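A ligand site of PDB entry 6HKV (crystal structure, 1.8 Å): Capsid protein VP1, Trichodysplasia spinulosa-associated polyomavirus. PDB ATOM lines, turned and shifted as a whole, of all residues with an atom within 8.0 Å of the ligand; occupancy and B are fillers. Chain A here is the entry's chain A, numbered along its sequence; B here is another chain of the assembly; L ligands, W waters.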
ATOM      1  N   LYS A  40       1.837 -15.369 -11.608  1.00  0.00           N
ATOM      2  CA  LYS A  40       0.639 -14.952 -12.329  1.00  0.00           C
ATOM      3  C   LYS A  40      -0.619 -15.391 -11.570  1.00  0.00           C
ATOM      4  O   LYS A  40      -0.735 -16.530 -11.129  1.00  0.00           O
ATOM      5  CB  LYS A  40       0.560 -15.550 -13.741  1.00  0.00           C
ATOM      6  CG  LYS A  40       1.689 -15.143 -14.699  1.00  0.00           C
ATOM      7  N   VAL A  41      -1.573 -14.457 -11.433  1.00  0.00           N
ATOM      8  CA  VAL A  41      -2.826 -14.710 -10.784  1.00  0.00           C
ATOM      9  C   VAL A  41      -3.679 -15.617 -11.686  1.00  0.00           C
ATOM     10  O   VAL A  41      -3.762 -15.399 -12.901  1.00  0.00           O
ATOM     11  CB  VAL A  41      -3.557 -13.392 -10.476  1.00  0.00           C
ATOM     12  CG1 VAL A  41      -5.001 -13.623 -10.022  1.00  0.00           C
ATOM     13  CG2 VAL A  41      -2.761 -12.590  -9.451  1.00  0.00           C
ATOM     14  N   THR A  42      -4.323 -16.602 -11.077  1.00  0.00           N
ATOM     15  CA  THR A  42      -5.291 -17.479 -11.737  1.00  0.00           C
ATOM     16  C   THR A  42      -6.647 -17.320 -11.036  1.00  0.00           C
ATOM     17  O   THR A  42      -6.730 -16.810  -9.915  1.00  0.00           O
ATOM     18  CB  THR A  42      -4.822 -18.937 -11.755  1.00  0.00           C
ATOM     19  OG1 THR A  42      -4.937 -19.512 -10.445  1.00  0.00           O
ATOM     20  CG2 THR A  42      -3.417 -19.081 -12.287  1.00  0.00           C
ATOM     21  N   VAL A  43      -7.711 -17.757 -11.727  1.00  0.00           N
ATOM     22  CA  VAL A  43      -9.058 -17.487 -11.281  1.00  0.00           C
ATOM     23  C   VAL A  43      -9.837 -18.807 -11.268  1.00  0.00           C
ATOM     24  O   VAL A  43      -9.860 -19.549 -12.253  1.00  0.00           O
ATOM     25  CB  VAL A  43      -9.730 -16.433 -12.182  1.00  0.00           C
ATOM     26  CG1 VAL A  43     -11.216 -16.269 -11.903  1.00  0.00           C
ATOM     27  CG2 VAL A  43      -8.986 -15.099 -12.119  1.00  0.00           C
ATOM     28  N   ALA A  44     -10.472 -19.091 -10.123  1.00  0.00           N
ATOM     29  CA  ALA A  44     -11.222 -20.304  -9.887  1.00  0.00           C
ATOM     30  C   ALA A  44     -12.352 -20.436 -10.914  1.00  0.00           C
ATOM     31  O   ALA A  44     -13.021 -19.462 -11.255  1.00  0.00           O
ATOM     32  CB  ALA A  44     -11.780 -20.267  -8.487  1.00  0.00           C
ATOM     33  N   ASN A  45     -12.566 -21.667 -11.375  1.00  0.00           N
ATOM     34  CA  ASN A  45     -13.731 -21.967 -12.251  1.00  0.00           C
ATOM     35  C   ASN A  45     -15.017 -21.893 -11.418  1.00  0.00           C
ATOM     36  O   ASN A  45     -16.049 -21.496 -11.900  1.00  0.00           O
ATOM     37  CB  ASN A  45     -13.605 -23.331 -12.937  1.00  0.00           C
ATOM     38  N   SER A  46     -14.935 -22.286 -10.145  1.00  0.00           N
ATOM     39  CA  SER A  46     -16.063 -22.243  -9.250  1.00  0.00           C
ATOM     40  C   SER A  46     -15.533 -22.176  -7.825  1.00  0.00           C
ATOM     41  O   SER A  46     -14.359 -22.505  -7.590  1.00  0.00           O
ATOM     42  CB  SER A  46     -16.948 -23.462  -9.429  1.00  0.00           C
ATOM     43  OG  SER A  46     -16.217 -24.648  -9.110  1.00  0.00           O
ATOM     44  N   ASP A  48     -15.989 -24.042  -5.321  1.00  0.00           N
ATOM     45  CA  ASP A  48     -15.594 -25.332  -4.765  1.00  0.00           C
ATOM     46  C   ASP A  48     -14.366 -25.903  -5.493  1.00  0.00           C
ATOM     47  O   ASP A  48     -13.940 -27.016  -5.181  1.00  0.00           O
ATOM     48  CB  ASP A  48     -16.762 -26.333  -4.787  1.00  0.00           C
ATOM     49  CG  ASP A  48     -17.278 -26.674  -6.179  1.00  0.00           C
ATOM     50  OD1 ASP A  48     -16.976 -25.929  -7.128  1.00  0.00           O
ATOM     51  OD2 ASP A  48     -17.937 -27.721  -6.300  1.00  0.00           O
ATOM     52  N   GLN A  49     -13.821 -25.164  -6.470  1.00  0.00           N
ATOM     53  CA  GLN A  49     -12.563 -25.520  -7.133  1.00  0.00           C
ATOM     54  C   GLN A  49     -11.655 -24.272  -7.160  1.00  0.00           C
ATOM     55  O   GLN A  49     -11.167 -23.872  -8.209  1.00  0.00           O
ATOM     56  CB  GLN A  49     -12.804 -26.040  -8.543  1.00  0.00           C
ATOM     57  CG  GLN A  49     -13.637 -27.323  -8.614  1.00  0.00           C
ATOM     58  CD  GLN A  49     -12.933 -28.517  -8.039  1.00  0.00           C
ATOM     59  OE1 GLN A  49     -11.743 -28.722  -8.262  1.00  0.00           O
ATOM     60  NE2 GLN A  49     -13.679 -29.340  -7.315  1.00  0.00           N
ATOM     61  N   ASP A  50     -11.457 -23.689  -5.975  1.00  0.00           N
ATOM     62  CA  ASP A  50     -10.711 -22.452  -5.804  1.00  0.00           C
ATOM     63  C   ASP A  50      -9.393 -22.822  -5.140  1.00  0.00           C
ATOM     64  O   ASP A  50      -9.312 -22.940  -3.917  1.00  0.00           O
ATOM     65  CB  ASP A  50     -11.551 -21.442  -5.008  1.00  0.00           C
ATOM     66  CG  ASP A  50     -10.938 -20.065  -4.906  1.00  0.00           C
ATOM     67  OD1 ASP A  50      -9.754 -19.908  -5.317  1.00  0.00           O
ATOM     68  OD2 ASP A  50     -11.667 -19.139  -4.432  1.00  0.00           O
ATOM     69  N   LYS A  51      -8.381 -23.041  -5.975  1.00  0.00           N
ATOM     70  CA  LYS A  51      -7.107 -23.598  -5.563  1.00  0.00           C
ATOM     71  C   LYS A  51      -5.994 -22.723  -6.137  1.00  0.00           C
ATOM     72  O   LYS A  51      -5.523 -22.939  -7.246  1.00  0.00           O
ATOM     73  CB  LYS A  51      -6.982 -25.058  -6.038  1.00  0.00           C
ATOM     74  CG  LYS A  51      -5.702 -25.736  -5.593  1.00  0.00           C
ATOM     75  N   PRO A  52      -5.558 -21.674  -5.419  1.00  0.00           N
ATOM     76  CA  PRO A  52      -4.496 -20.835  -5.911  1.00  0.00           C
ATOM     77  C   PRO A  52      -3.230 -21.651  -6.234  1.00  0.00           C
ATOM     78  O   PRO A  52      -2.862 -22.557  -5.497  1.00  0.00           O
ATOM     79  CB  PRO A  52      -4.239 -19.806  -4.812  1.00  0.00           C
ATOM     80  CG  PRO A  52      -5.023 -20.256  -3.644  1.00  0.00           C
ATOM     81  CD  PRO A  52      -6.079 -21.207  -4.135  1.00  0.00           C
ATOM     82  N   THR A  53      -2.579 -21.274  -7.341  1.00  0.00           N
ATOM     83  CA  THR A  53      -1.308 -21.854  -7.703  1.00  0.00           C
ATOM     84  C   THR A  53      -0.272 -21.465  -6.647  1.00  0.00           C
ATOM     85  O   THR A  53      -0.404 -20.467  -5.906  1.00  0.00           O
ATOM     86  CB  THR A  53      -0.885 -21.415  -9.098  1.00  0.00           C
ATOM     87  OG1 THR A  53      -0.732 -19.980  -9.130  1.00  0.00           O
ATOM     88  CG2 THR A  53      -1.878 -21.849 -10.141  1.00  0.00           C
ATOM     89  N   SER A  54       0.790 -22.275  -6.578  1.00  0.00           N
ATOM     90  CA  SER A  54       1.897 -22.009  -5.699  1.00  0.00           C
ATOM     91  C   SER A  54       2.540 -20.679  -6.098  1.00  0.00           C
ATOM     92  O   SER A  54       2.923 -20.478  -7.256  1.00  0.00           O
ATOM     93  CB  SER A  54       2.909 -23.116  -5.733  1.00  0.00           C
ATOM     94  OG  SER A  54       3.883 -22.899  -4.734  1.00  0.00           O
ATOM     95  N   GLU A  56       1.159 -17.559  -5.973  1.00  0.00           N
ATOM     96  CA  GLU A  56       0.321 -16.435  -6.465  1.00  0.00           C
ATOM     97  C   GLU A  56      -0.329 -15.643  -5.315  1.00  0.00           C
ATOM     98  O   GLU A  56      -1.083 -14.731  -5.585  1.00  0.00           O
ATOM     99  CB  GLU A  56      -0.723 -16.876  -7.497  1.00  0.00           C
ATOM    100  CG  GLU A  56      -1.956 -17.540  -6.946  1.00  0.00           C
ATOM    101  CD  GLU A  56      -3.030 -17.679  -8.004  1.00  0.00           C
ATOM    102  OE1 GLU A  56      -3.094 -18.752  -8.670  1.00  0.00           O
ATOM    103  OE2 GLU A  56      -3.806 -16.697  -8.167  1.00  0.00           O
ATOM    104  N   ILE A  57      -0.018 -15.973  -4.080  1.00  0.00           N
ATOM    105  CA  ILE A  57      -0.710 -15.434  -2.904  1.00  0.00           C
ATOM    106  C   ILE A  57       0.248 -14.631  -2.015  1.00  0.00           C
ATOM    107  O   ILE A  57       1.189 -15.197  -1.486  1.00  0.00           O
ATOM    108  CB  ILE A  57      -1.226 -16.682  -2.129  1.00  0.00           C
ATOM    109  CG1 ILE A  57      -2.388 -17.412  -2.813  1.00  0.00           C
ATOM    110  CG2 ILE A  57      -1.614 -16.383  -0.706  1.00  0.00           C
ATOM    111  CD1 ILE A  57      -3.438 -16.480  -3.235  1.00  0.00           C
ATOM    112  N   THR A 143     -11.439 -22.268   0.017  1.00  0.00           N
ATOM    113  CA  THR A 143     -10.176 -22.076  -0.670  1.00  0.00           C
ATOM    114  C   THR A 143      -9.211 -23.208  -0.295  1.00  0.00           C
ATOM    115  O   THR A 143      -9.029 -23.517   0.881  1.00  0.00           O
ATOM    116  CB  THR A 143      -9.515 -20.717  -0.351  1.00  0.00           C
ATOM    117  OG1 THR A 143     -10.513 -19.712  -0.547  1.00  0.00           O
ATOM    118  CG2 THR A 143      -8.332 -20.429  -1.250  1.00  0.00           C
ATOM    119  N   ASP A 144      -8.583 -23.784  -1.326  1.00  0.00           N
ATOM    120  CA  ASP A 144      -7.705 -24.936  -1.173  1.00  0.00           C
ATOM    121  C   ASP A 144      -6.258 -24.465  -1.355  1.00  0.00           C
ATOM    122  O   ASP A 144      -5.874 -24.098  -2.464  1.00  0.00           O
ATOM    123  CB  ASP A 144      -8.106 -25.999  -2.211  1.00  0.00           C
ATOM    124  CG  ASP A 144      -7.189 -27.209  -2.281  1.00  0.00           C
ATOM    125  OD1 ASP A 144      -6.233 -27.308  -1.425  1.00  0.00           O
ATOM    126  OD2 ASP A 144      -7.442 -28.035  -3.174  1.00  0.00           O
ATOM    127  N   ALA A 147      -1.679 -26.496  -3.006  1.00  0.00           N
ATOM    128  CA  ALA A 147      -0.604 -26.365  -4.018  1.00  0.00           C
ATOM    129  C   ALA A 147       0.703 -25.863  -3.383  1.00  0.00           C
ATOM    130  O   ALA A 147       1.755 -25.958  -3.984  1.00  0.00           O
ATOM    131  CB  ALA A 147      -1.026 -25.447  -5.140  1.00  0.00           C
ATOM    132  N   ASN B  99      -7.863 -10.545  -2.502  1.00  0.00           N
ATOM    133  CA  ASN B  99      -8.192 -11.864  -3.053  1.00  0.00           C
ATOM    134  C   ASN B  99      -8.791 -11.627  -4.421  1.00  0.00           C
ATOM    135  O   ASN B  99      -9.907 -11.089  -4.521  1.00  0.00           O
ATOM    136  CB  ASN B  99      -9.127 -12.655  -2.138  1.00  0.00           C
ATOM    137  CG  ASN B  99      -9.379 -14.077  -2.599  1.00  0.00           C
ATOM    138  OD1 ASN B  99      -9.180 -14.385  -3.768  1.00  0.00           O
ATOM    139  ND2 ASN B  99      -9.808 -14.926  -1.684  1.00  0.00           N
ATOM    140  N   VAL B 100      -8.049 -12.046  -5.458  1.00  0.00           N
ATOM    141  CA  VAL B 100      -8.490 -11.865  -6.822  1.00  0.00           C
ATOM    142  C   VAL B 100      -8.418 -13.193  -7.592  1.00  0.00           C
ATOM    143  O   VAL B 100      -8.301 -13.172  -8.823  1.00  0.00           O
ATOM    144  CB  VAL B 100      -7.672 -10.777  -7.531  1.00  0.00           C
ATOM    145  CG1 VAL B 100      -8.022  -9.402  -6.976  1.00  0.00           C
ATOM    146  CG2 VAL B 100      -6.167 -11.025  -7.487  1.00  0.00           C
ATOM    147  N   HIS B 101      -8.517 -14.319  -6.887  1.00  0.00           N
ATOM    148  CA  HIS B 101      -8.535 -15.646  -7.539  1.00  0.00           C
ATOM    149  C   HIS B 101      -9.845 -16.382  -7.309  1.00  0.00           C
ATOM    150  O   HIS B 101      -9.971 -17.576  -7.671  1.00  0.00           O
ATOM    151  CB  HIS B 101      -7.347 -16.502  -7.078  1.00  0.00           C
ATOM    152  CG  HIS B 101      -7.286 -16.717  -5.614  1.00  0.00           C
ATOM    153  ND1 HIS B 101      -8.148 -17.567  -4.946  1.00  0.00           N
ATOM    154  CD2 HIS B 101      -6.479 -16.183  -4.671  1.00  0.00           C
ATOM    155  CE1 HIS B 101      -7.859 -17.551  -3.655  1.00  0.00           C
ATOM    156  NE2 HIS B 101      -6.842 -16.696  -3.467  1.00  0.00           N
ATOM    157  N   MET B 102     -10.837 -15.721  -6.703  1.00  0.00           N
ATOM    158  CA  MET B 102     -12.150 -16.343  -6.504  1.00  0.00           C
ATOM    159  C   MET B 102     -12.854 -16.443  -7.857  1.00  0.00           C
ATOM    160  O   MET B 102     -12.455 -15.821  -8.843  1.00  0.00           O
ATOM    161  CB  MET B 102     -13.006 -15.560  -5.508  1.00  0.00           C
ATOM    162  CG  MET B 102     -12.497 -15.680  -4.092  1.00  0.00           C
ATOM    163  SD  MET B 102     -13.565 -14.867  -2.882  1.00  0.00           S
ATOM    164  CE  MET B 102     -13.336 -13.147  -3.346  1.00  0.00           C
ATOM    165  N   ALA B 103     -13.892 -17.278  -7.917  1.00  0.00           N
ATOM    166  CA  ALA B 103     -14.641 -17.502  -9.156  1.00  0.00           C
ATOM    167  C   ALA B 103     -15.516 -16.279  -9.442  1.00  0.00           C
ATOM    168  O   ALA B 103     -16.681 -16.212  -9.048  1.00  0.00           O
ATOM    169  CB  ALA B 103     -15.461 -18.763  -9.057  1.00  0.00           C
ATOM    170  N   ARG B 106     -13.444 -11.424 -14.645  1.00  0.00           N
ATOM    171  CA  ARG B 106     -12.028 -11.117 -14.576  1.00  0.00           C
ATOM    172  C   ARG B 106     -11.654 -10.091 -15.632  1.00  0.00           C
ATOM    173  O   ARG B 106     -12.405  -9.807 -16.575  1.00  0.00           O
ATOM    174  CB  ARG B 106     -11.212 -12.419 -14.580  1.00  0.00           C
ATOM    175  CG  ARG B 106     -11.207 -13.184 -15.856  1.00  0.00           C
ATOM    176  CD  ARG B 106     -10.576 -14.570 -15.659  1.00  0.00           C
ATOM    177  NE  ARG B 106      -9.129 -14.453 -15.459  1.00  0.00           N
ATOM    178  CZ  ARG B 106      -8.280 -15.478 -15.424  1.00  0.00           C
ATOM    179  NH1 ARG B 106      -7.011 -15.276 -15.116  1.00  0.00           N
ATOM    180  NH2 ARG B 106      -8.698 -16.718 -15.659  1.00  0.00           N
ATOM    181  N   ASP B 110     -10.291 -12.383 -19.980  1.00  0.00           N
ATOM    182  CA  ASP B 110     -10.200 -13.631 -19.224  1.00  0.00           C
ATOM    183  C   ASP B 110      -8.762 -14.049 -18.935  1.00  0.00           C
ATOM    184  O   ASP B 110      -8.532 -15.202 -18.596  1.00  0.00           O
ATOM    185  CB  ASP B 110     -11.027 -14.735 -19.875  1.00  0.00           C
ATOM    186  CG  ASP B 110     -12.514 -14.512 -19.721  1.00  0.00           C
ATOM    187  OD1 ASP B 110     -12.933 -13.985 -18.698  1.00  0.00           O
ATOM    188  OD2 ASP B 110     -13.264 -14.828 -20.635  1.00  0.00           O
HETATM  189  C1  LIG L   1      -6.373 -22.445 -12.550  1.00  0.00           C
HETATM  190  C2  LIG L   1      -7.784 -21.978 -12.916  1.00  0.00           C
HETATM  191  C3  LIG L   1      -9.064 -21.009 -14.892  1.00  0.00           C
HETATM  192  O1  LIG L   1      -4.332 -25.018 -14.315  1.00  0.00           O
HETATM  193  C4  LIG L   1      -7.623 -20.307  -8.405  1.00  0.00           C
HETATM  194  C5  LIG L   1      -7.521 -21.629  -9.202  1.00  0.00           C
HETATM  195  O2  LIG L   1      -8.301 -22.561  -8.892  1.00  0.00           O
HETATM  196  N1  LIG L   1      -6.544 -21.683 -10.168  1.00  0.00           N
HETATM  197  C6  LIG L   1      -6.302 -22.840 -11.076  1.00  0.00           C
HETATM  198  C7  LIG L   1      -4.962 -23.518 -10.782  1.00  0.00           C
HETATM  199  C8  LIG L   1      -4.554 -24.566 -11.846  1.00  0.00           C
HETATM  200  C9  LIG L   1      -4.618 -24.010 -13.307  1.00  0.00           C
HETATM  201  O3  LIG L   1      -5.975 -23.545 -13.440  1.00  0.00           O
HETATM  202  C10 LIG L   1      -7.829 -21.778 -14.426  1.00  0.00           C
HETATM  203  O4  LIG L   1      -9.013 -20.975 -16.331  1.00  0.00           O
HETATM  204  O5  LIG L   1      -6.654 -21.049 -14.829  1.00  0.00           O
HETATM  205  O6  LIG L   1      -8.791 -22.915 -12.419  1.00  0.00           O
HETATM  206  C11 LIG L   1      -3.608 -22.932 -13.677  1.00  0.00           C
HETATM  207  O7  LIG L   1      -3.889 -21.992 -14.474  1.00  0.00           O
HETATM  208  O8  LIG L   1      -2.460 -23.043 -13.217  1.00  0.00           O
HETATM  209  O9  LIG L   1      -5.079 -24.096  -9.480  1.00  0.00           O
HETATM  210  O   HOH W   1      -6.563 -18.591 -14.528  1.00  0.00           O
HETATM  211  O   HOH W   2      -0.468 -20.457 -13.332  1.00  0.00           O
HETATM  212  O   HOH W   3      -0.302 -24.357 -12.823  1.00  0.00           O
HETATM  213  O   HOH W   4     -10.735 -23.757 -10.700  1.00  0.00           O
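O of Lys 51 sits at hydrogen-bond distance from O9 of the ligand, 2.6 Å away.
A nitrogen (N1) of the ligand sits at hydrogen-bond distance from the side-chain hydroxyl (OG1) of Thr 42, 2.7 Å away.
An oxygen (O2) of the ligand lies within hydrogen-bond range of the backbone NH (N) of Lys 51, at 3.0 Å.
The side-chain carboxylate (OE1) of Glu 56 is in hydrogen-bond range of the side-chain hydroxyl (OG1) of Thr 42.
The backbone carbonyl oxygen (O) of Asp 50 lies within hydrogen-bond range of the backbone NH (N) of Asp 144.
The backbone NH (N) of Ala 44 sits at hydrogen-bond distance from the backbone carbonyl oxygen (O) of His 101 of chain B (2.9 Å).
OG1 of Thr 53 sits at hydrogen-bond distance from OE1 of Glu 56 (2.7 Å).
ND1 of His 101 of chain B sits at hydrogen-bond distance from OD1 of Asp 50 (2.9 Å).
OD1 of Asn 99 of chain B is in hydrogen-bond range of N of His 101 of chain B.
O of Gln 49 sits close to O2 of the ligand (3.2 Å).
Val 43 touches the ligand (O to C3, 3.1 Å).
N of Ala 44 touches C4 of the ligand, at 3.5 Å.
OD1 of Asp 50 touches C4 of the ligand, at 3.8 Å.
Pro 52 touches the ligand.
CG2 of Thr 53 touches O8 of the ligand, at 3.4 Å.
O of His 101 of chain B touches C4 of the ligand, at 3.7 Å.
Of the 26 residues printed, 9 come within 4 Å of the ligand.
The nearest printed residue that does not touch the ligand is Asn 45 (4.1 Å).
Water W1 lies within hydrogen-bond range of an oxygen (O5) of the ligand (2.5 Å), the guanidinium group (NH2) of Arg 106 of chain B (3.1 Å) and the backbone NH (N) of Val 43 (3.1 Å).
Water W4 lies within hydrogen-bond range of the backbone carbonyl oxygen (O) of Gln 49, an oxygen (O6) of the ligand and the backbone NH (N) of Asn 45.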
